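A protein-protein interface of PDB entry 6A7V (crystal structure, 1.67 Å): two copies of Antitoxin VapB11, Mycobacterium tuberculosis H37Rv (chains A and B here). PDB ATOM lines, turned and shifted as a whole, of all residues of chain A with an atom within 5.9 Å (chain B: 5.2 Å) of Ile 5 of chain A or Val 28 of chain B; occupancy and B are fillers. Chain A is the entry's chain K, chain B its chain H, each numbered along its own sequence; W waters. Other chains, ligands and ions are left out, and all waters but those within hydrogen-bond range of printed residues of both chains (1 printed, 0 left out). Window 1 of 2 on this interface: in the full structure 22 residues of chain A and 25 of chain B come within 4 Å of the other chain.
The side-chain amide oxygen of Asn 4 of chain A sits close to the backbone carbonyl oxygen of Thr 3 of chain B, at 3.0 Å.
O of Thr 3 of chain B sits at hydrogen-bond distance from N of Ile 5 of chain A, 3.2 Å away.
OD1 of Asp 6 of chain A is in salt-bridge range of NH1 of Arg 25 of chain B.
The backbone carbonyl oxygen of Ser 1 of chain B is in hydrogen-bond range of the backbone NH of Ile 7 of chain A (2.9 Å).
O of Ser 1 of chain B sits at hydrogen-bond distance from OG1 of Thr 3 of chain B (2.6 Å).
The guanidinium group (NE) of Arg 25 of chain B is in salt-bridge range of the side-chain carboxylate (OD1) of Asp 29 of chain B, 3.7 Å away.
Asn 4 of chain A touches Arg 2 of chain B.
Ile 5 of chain A touches Ser 1 of chain B.
Ile 5 of chain A touches Val 28 of chain B (CD1 to CG2, 3.9 Å).
Asp 6 of chain A touches Ser 1 of chain B (CA to O, 3.3 Å).
Ile 7 of chain A touches Thr 3 of chain B.
Ile 7 of chain A touches Leu 32 of chain B.
Ala 31 of chain A touches Leu 32 of chain B.
Ile 7 of chain B touches Leu 32 of chain A (CG2 to CD1, 3.9 Å).
Leu 32 of chain A touches Ala 27 of chain B (CD2 to O, 3.7 Å).
Ala 31 of chain B touches Leu 32 of chain A.
Of chain B, only Ser 1, Thr 3, Ile 7 and Val 28 come within 4 Å of Ile 5 of chain A.
Val 28 of chain B touches just one residue of chain A: Ile 5.
Of the printed residues of chain A, Arg 2 of chain B touches Asn 4 (3.7 Å) and Asp 6 (3.2 Å).
Of the printed residues of chain A, Ser 1 of chain B touches Ile 5, Asp 6 and Ile 7.
Leu 30 of chain B touches none of the printed residues of chain A.
The nearest residue of chain B that does not touch Ile 5 of chain A is Arg 2 of chain B (4.2 Å).
The nearest residue of chain A that does not touch Val 28 of chain B is Leu 32 of chain A (4.1 Å).
Hydrophobic or aromatic side chains of chain A within 4 Å of the printed part of chain B: Ile 5, Ile 7, Ala 31 and Leu 32.
Printed residues of chain B that touch a printed residue of chain A: Ser 1, Arg 2, Thr 3, Ile 7, Arg 25, Ala 27, Val 28, Ala 31 and Leu 32.
Among the printed residues, 18 pairs touch across the chains.
Ile 7 of chain A touches Thr 3 of chain B, but with the chains exchanged Thr 3 of chain A does not touch Ile 7 of chain B (4.7 Å).
Ile 7 of chain A touches Leu 32 of chain B, and with the chains exchanged Leu 32 of chain A touches Ile 7 of chain B.
Ala 31 of chain A touches its own counterpart, Ala 31 of chain B.
Ala 31 of chain A touches Leu 32 of chain B, and with the chains exchanged Leu 32 of chain A touches Ala 31 of chain B.
Of the 18 pairs that touch across the chains among the printed residues, 6 have their exchanged pair printed and touching as well.
Water W1 lies within hydrogen-bond range of O of Ala 31 of chain B (2.8 Å) and O of Ala 31 of chain A (2.9 Å).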
ATOM      1  N   THR A   3      -5.416  25.811 -20.480  1.00  0.00           N
ATOM      2  CA  THR A   3      -4.995  24.728 -21.367  1.00  0.00           C
ATOM      3  C   THR A   3      -5.975  23.566 -21.290  1.00  0.00           C
ATOM      4  O   THR A   3      -6.436  23.204 -20.206  1.00  0.00           O
ATOM      5  CB  THR A   3      -3.593  24.199 -20.997  1.00  0.00           C
ATOM      6  OG1 THR A   3      -2.711  25.295 -20.725  1.00  0.00           O
ATOM      7  CG2 THR A   3      -3.020  23.359 -22.134  1.00  0.00           C
ATOM      8  N   ASN A   4      -6.284  22.988 -22.447  1.00  0.00           N
ATOM      9  CA  ASN A   4      -7.101  21.786 -22.522  1.00  0.00           C
ATOM     10  C   ASN A   4      -6.182  20.583 -22.730  1.00  0.00           C
ATOM     11  O   ASN A   4      -5.632  20.394 -23.817  1.00  0.00           O
ATOM     12  CB  ASN A   4      -8.114  21.901 -23.670  1.00  0.00           C
ATOM     13  CG  ASN A   4      -9.172  20.807 -23.639  1.00  0.00           C
ATOM     14  OD1 ASN A   4      -9.243  20.006 -22.702  1.00  0.00           O
ATOM     15  ND2 ASN A   4     -10.010  20.773 -24.671  1.00  0.00           N
ATOM     16  N   ILE A   5      -5.999  19.791 -21.675  1.00  0.00           N
ATOM     17  CA  ILE A   5      -5.229  18.549 -21.762  1.00  0.00           C
ATOM     18  C   ILE A   5      -5.974  17.398 -21.097  1.00  0.00           C
ATOM     19  O   ILE A   5      -6.723  17.602 -20.140  1.00  0.00           O
ATOM     20  CB  ILE A   5      -3.822  18.675 -21.135  1.00  0.00           C
ATOM     21  CG1 ILE A   5      -3.889  19.297 -19.737  1.00  0.00           C
ATOM     22  CG2 ILE A   5      -2.910  19.494 -22.038  1.00  0.00           C
ATOM     23  CD1 ILE A   5      -2.647  19.043 -18.912  1.00  0.00           C
ATOM     24  N   ASP A   6      -5.762  16.193 -21.619  1.00  0.00           N
ATOM     25  CA  ASP A   6      -6.367  14.993 -21.060  1.00  0.00           C
ATOM     26  C   ASP A   6      -5.769  14.720 -19.687  1.00  0.00           C
ATOM     27  O   ASP A   6      -4.579  14.438 -19.569  1.00  0.00           O
ATOM     28  CB  ASP A   6      -6.142  13.790 -21.983  1.00  0.00           C
ATOM     29  CG  ASP A   6      -6.760  12.503 -21.446  1.00  0.00           C
ATOM     30  OD1 ASP A   6      -6.222  11.934 -20.472  1.00  0.00           O
ATOM     31  OD2 ASP A   6      -7.776  12.049 -22.015  1.00  0.00           O
ATOM     32  N   ILE A   7      -6.599  14.828 -18.656  1.00  0.00           N
ATOM     33  CA  ILE A   7      -6.214  14.441 -17.306  1.00  0.00           C
ATOM     34  C   ILE A   7      -7.194  13.372 -16.852  1.00  0.00           C
ATOM     35  O   ILE A   7      -8.402  13.577 -16.916  1.00  0.00           O
ATOM     36  CB  ILE A   7      -6.246  15.643 -16.340  1.00  0.00           C
ATOM     37  CG1 ILE A   7      -5.186  16.670 -16.749  1.00  0.00           C
ATOM     38  CG2 ILE A   7      -6.007  15.191 -14.903  1.00  0.00           C
ATOM     39  CD1 ILE A   7      -5.468  18.069 -16.254  1.00  0.00           C
ATOM     40  N   VAL A  28      -4.110  19.544  -9.556  1.00  0.00           N
ATOM     41  CA  VAL A  28      -3.008  19.450 -10.529  1.00  0.00           C
ATOM     42  C   VAL A  28      -1.915  20.418 -10.149  1.00  0.00           C
ATOM     43  O   VAL A  28      -0.727  20.049 -10.203  1.00  0.00           O
ATOM     44  CB  VAL A  28      -3.477  19.726 -11.975  1.00  0.00           C
ATOM     45  CG1 VAL A  28      -2.292  19.938 -12.917  1.00  0.00           C
ATOM     46  CG2 VAL A  28      -4.342  18.578 -12.474  1.00  0.00           C
ATOM     47  N   ALA A  31      -0.005  19.069  -7.247  1.00  0.00           N
ATOM     48  CA  ALA A  31       0.844  17.959  -7.656  1.00  0.00           C
ATOM     49  C   ALA A  31       2.098  18.511  -8.354  1.00  0.00           C
ATOM     50  O   ALA A  31       3.179  18.011  -8.121  1.00  0.00           O
ATOM     51  CB  ALA A  31       0.082  17.008  -8.565  1.00  0.00           C
ATOM     52  N   LEU A  32       1.946  19.548  -9.183  1.00  0.00           N
ATOM     53  CA  LEU A  32       3.088  20.075  -9.870  1.00  0.00           C
ATOM     54  C   LEU A  32       4.074  20.719  -8.849  1.00  0.00           C
ATOM     55  O   LEU A  32       5.282  20.547  -8.899  1.00  0.00           O
ATOM     56  CB  LEU A  32       2.676  21.080 -10.948  1.00  0.00           C
ATOM     57  CG  LEU A  32       2.098  20.454 -12.222  1.00  0.00           C
ATOM     58  CD1 LEU A  32       1.371  21.501 -13.051  1.00  0.00           C
ATOM     59  CD2 LEU A  32       3.186  19.784 -13.050  1.00  0.00           C
ATOM     60  N   SER B   1     -12.154  13.346 -19.556  1.00  0.00           N
ATOM     61  CA  SER B   1     -10.756  13.450 -19.258  1.00  0.00           C
ATOM     62  C   SER B   1     -10.197  14.615 -20.019  1.00  0.00           C
ATOM     63  O   SER B   1      -9.277  15.232 -19.560  1.00  0.00           O
ATOM     64  CB  SER B   1     -10.043  12.136 -19.481  1.00  0.00           C
ATOM     65  OG  SER B   1     -10.569  11.165 -18.574  1.00  0.00           O
ATOM     66  N   ARG B   2     -10.803  14.958 -21.147  1.00  0.00           N
ATOM     67  CA  ARG B   2     -10.372  16.138 -21.859  1.00  0.00           C
ATOM     68  C   ARG B   2     -10.843  17.181 -20.873  1.00  0.00           C
ATOM     69  O   ARG B   2     -12.018  17.286 -20.579  1.00  0.00           O
ATOM     70  CB  ARG B   2     -11.100  16.218 -23.170  1.00  0.00           C
ATOM     71  CG  ARG B   2     -10.880  14.955 -23.948  1.00  0.00           C
ATOM     72  CD  ARG B   2      -9.389  14.731 -24.147  1.00  0.00           C
ATOM     73  NE  ARG B   2      -8.767  15.928 -24.698  1.00  0.00           N
ATOM     74  CZ  ARG B   2      -7.501  16.016 -25.058  1.00  0.00           C
ATOM     75  NH1 ARG B   2      -6.701  14.972 -24.938  1.00  0.00           N
ATOM     76  NH2 ARG B   2      -7.039  17.150 -25.542  1.00  0.00           N
ATOM     77  N   THR B   3      -9.902  17.963 -20.379  1.00  0.00           N
ATOM     78  CA  THR B   3     -10.183  18.838 -19.286  1.00  0.00           C
ATOM     79  C   THR B   3      -9.652  20.197 -19.497  1.00  0.00           C
ATOM     80  O   THR B   3      -8.508  20.394 -19.800  1.00  0.00           O
ATOM     81  CB  THR B   3      -9.527  18.270 -18.025  1.00  0.00           C
ATOM     82  OG1 THR B   3     -10.016  16.947 -17.781  1.00  0.00           O
ATOM     83  CG2 THR B   3      -9.854  19.116 -16.857  1.00  0.00           C
ATOM     84  N   ILE B   7      -3.385  25.895 -15.976  1.00  0.00           N
ATOM     85  CA  ILE B   7      -2.141  25.327 -15.469  1.00  0.00           C
ATOM     86  C   ILE B   7      -1.052  26.386 -15.553  1.00  0.00           C
ATOM     87  O   ILE B   7      -0.795  26.936 -16.624  1.00  0.00           O
ATOM     88  CB  ILE B   7      -1.712  24.081 -16.266  1.00  0.00           C
ATOM     89  CG1 ILE B   7      -2.721  22.950 -16.052  1.00  0.00           C
ATOM     90  CG2 ILE B   7      -0.322  23.622 -15.842  1.00  0.00           C
ATOM     91  CD1 ILE B   7      -2.592  21.817 -17.044  1.00  0.00           C
ATOM     92  N   LYS B  24       4.269  19.062 -21.162  1.00  0.00           N
ATOM     93  CA  LYS B  24       3.433  19.543 -20.104  1.00  0.00           C
ATOM     94  C   LYS B  24       2.649  18.289 -19.766  1.00  0.00           C
ATOM     95  O   LYS B  24       2.403  18.011 -18.630  1.00  0.00           O
ATOM     96  CB  LYS B  24       2.579  20.696 -20.570  1.00  0.00           C
ATOM     97  CG  LYS B  24       3.403  21.956 -20.718  1.00  0.00           C
ATOM     98  CD  LYS B  24       2.560  23.221 -20.793  1.00  0.00           C
ATOM     99  CE  LYS B  24       3.355  24.416 -21.316  1.00  0.00           C
ATOM    100  NZ  LYS B  24       4.556  24.701 -20.495  1.00  0.00           N
ATOM    101  N   ARG B  25       2.270  17.534 -20.777  1.00  0.00           N
ATOM    102  CA  ARG B  25       1.625  16.266 -20.622  1.00  0.00           C
ATOM    103  C   ARG B  25       2.626  15.470 -19.790  1.00  0.00           C
ATOM    104  O   ARG B  25       2.255  14.693 -18.957  1.00  0.00           O
ATOM    105  CB  ARG B  25       1.454  15.588 -21.971  1.00  0.00           C
ATOM    106  CG  ARG B  25       0.676  14.282 -21.935  1.00  0.00           C
ATOM    107  CD  ARG B  25      -0.828  14.508 -21.844  1.00  0.00           C
ATOM    108  NE  ARG B  25      -1.468  13.383 -21.183  1.00  0.00           N
ATOM    109  CZ  ARG B  25      -2.395  12.574 -21.703  1.00  0.00           C
ATOM    110  NH1 ARG B  25      -2.868  11.576 -20.980  1.00  0.00           N
ATOM    111  NH2 ARG B  25      -2.862  12.755 -22.920  1.00  0.00           N
ATOM    112  N   ALA B  26       3.915  15.614 -20.065  1.00  0.00           N
ATOM    113  CA  ALA B  26       4.882  14.883 -19.269  1.00  0.00           C
ATOM    114  C   ALA B  26       4.936  15.330 -17.816  1.00  0.00           C
ATOM    115  O   ALA B  26       5.032  14.503 -16.939  1.00  0.00           O
ATOM    116  CB  ALA B  26       6.267  14.936 -19.880  1.00  0.00           C
ATOM    117  N   ALA B  27       4.916  16.636 -17.581  1.00  0.00           N
ATOM    118  CA  ALA B  27       4.981  17.147 -16.237  1.00  0.00           C
ATOM    119  C   ALA B  27       3.784  16.807 -15.393  1.00  0.00           C
ATOM    120  O   ALA B  27       3.922  16.399 -14.270  1.00  0.00           O
ATOM    121  CB  ALA B  27       5.201  18.636 -16.247  1.00  0.00           C
ATOM    122  N   VAL B  28       2.600  16.967 -15.951  1.00  0.00           N
ATOM    123  CA  VAL B  28       1.355  16.703 -15.222  1.00  0.00           C
ATOM    124  C   VAL B  28       1.238  15.202 -14.896  1.00  0.00           C
ATOM    125  O   VAL B  28       0.919  14.843 -13.767  1.00  0.00           O
ATOM    126  CB  VAL B  28       0.110  17.172 -16.011  1.00  0.00           C
ATOM    127  CG1 VAL B  28      -1.174  16.681 -15.351  1.00  0.00           C
ATOM    128  CG2 VAL B  28       0.092  18.689 -16.123  1.00  0.00           C
ATOM    129  N   ASP B  29       1.554  14.385 -15.902  1.00  0.00           N
ATOM    130  CA  ASP B  29       1.467  12.947 -15.783  1.00  0.00           C
ATOM    131  C   ASP B  29       2.345  12.546 -14.615  1.00  0.00           C
ATOM    132  O   ASP B  29       1.879  11.885 -13.723  1.00  0.00           O
ATOM    133  CB  ASP B  29       1.950  12.209 -17.043  1.00  0.00           C
ATOM    134  CG  ASP B  29       0.829  11.932 -18.045  1.00  0.00           C
ATOM    135  OD1 ASP B  29      -0.320  12.368 -17.823  1.00  0.00           O
ATOM    136  OD2 ASP B  29       1.109  11.268 -19.068  1.00  0.00           O
ATOM    137  N   LEU B  30       3.608  12.968 -14.645  1.00  0.00           N
ATOM    138  CA  LEU B  30       4.561  12.600 -13.610  1.00  0.00           C
ATOM    139  C   LEU B  30       3.997  13.053 -12.260  1.00  0.00           C
ATOM    140  O   LEU B  30       3.841  12.248 -11.396  1.00  0.00           O
ATOM    141  CB  LEU B  30       5.918  13.263 -13.862  1.00  0.00           C
ATOM    142  CG  LEU B  30       6.982  13.114 -12.768  1.00  0.00           C
ATOM    143  CD1 LEU B  30       7.320  11.649 -12.542  1.00  0.00           C
ATOM    144  CD2 LEU B  30       8.229  13.911 -13.118  1.00  0.00           C
ATOM    145  N   ALA B  31       3.641  14.345 -12.190  1.00  0.00           N
ATOM    146  CA  ALA B  31       3.154  14.960 -10.994  1.00  0.00           C
ATOM    147  C   ALA B  31       2.077  14.075 -10.343  1.00  0.00           C
ATOM    148  O   ALA B  31       2.009  13.981  -9.133  1.00  0.00           O
ATOM    149  CB  ALA B  31       2.602  16.348 -11.282  1.00  0.00           C
ATOM    150  N   LEU B  32       1.174  13.547 -11.168  1.00  0.00           N
ATOM    151  CA  LEU B  32       0.065  12.792 -10.669  1.00  0.00           C
ATOM    152  C   LEU B  32       0.506  11.367 -10.283  1.00  0.00           C
ATOM    153  O   LEU B  32       0.043  10.835  -9.283  1.00  0.00           O
ATOM    154  CB  LEU B  32      -1.113  12.781 -11.655  1.00  0.00           C
ATOM    155  CG  LEU B  32      -1.835  14.126 -11.828  1.00  0.00           C
ATOM    156  CD1 LEU B  32      -2.954  13.988 -12.850  1.00  0.00           C
ATOM    157  CD2 LEU B  32      -2.380  14.663 -10.511  1.00  0.00           C
ATOM    158  N   ARG B  33       1.317  10.754 -11.107  1.00  0.00           N
ATOM    159  CA  ARG B  33       1.761   9.405 -10.857  1.00  0.00           C
ATOM    160  C   ARG B  33       2.524   9.313  -9.541  1.00  0.00           C
ATOM    161  O   ARG B  33       2.333   8.368  -8.787  1.00  0.00           O
ATOM    162  CB  ARG B  33       2.654   8.925 -12.015  1.00  0.00           C
ATOM    163  CG  ARG B  33       3.147   7.484 -11.898  1.00  0.00           C
ATOM    164  CD  ARG B  33       4.421   7.235 -12.699  1.00  0.00           C
ATOM    165  NE  ARG B  33       5.250   6.182 -12.101  1.00  0.00           N
ATOM    166  CZ  ARG B  33       6.096   6.354 -11.081  1.00  0.00           C
ATOM    167  NH1 ARG B  33       6.793   5.319 -10.620  1.00  0.00           N
ATOM    168  NH2 ARG B  33       6.251   7.546 -10.505  1.00  0.00           N
HETATM  169  O   HOH W   1       3.484  15.326  -7.168  1.00  0.00           O
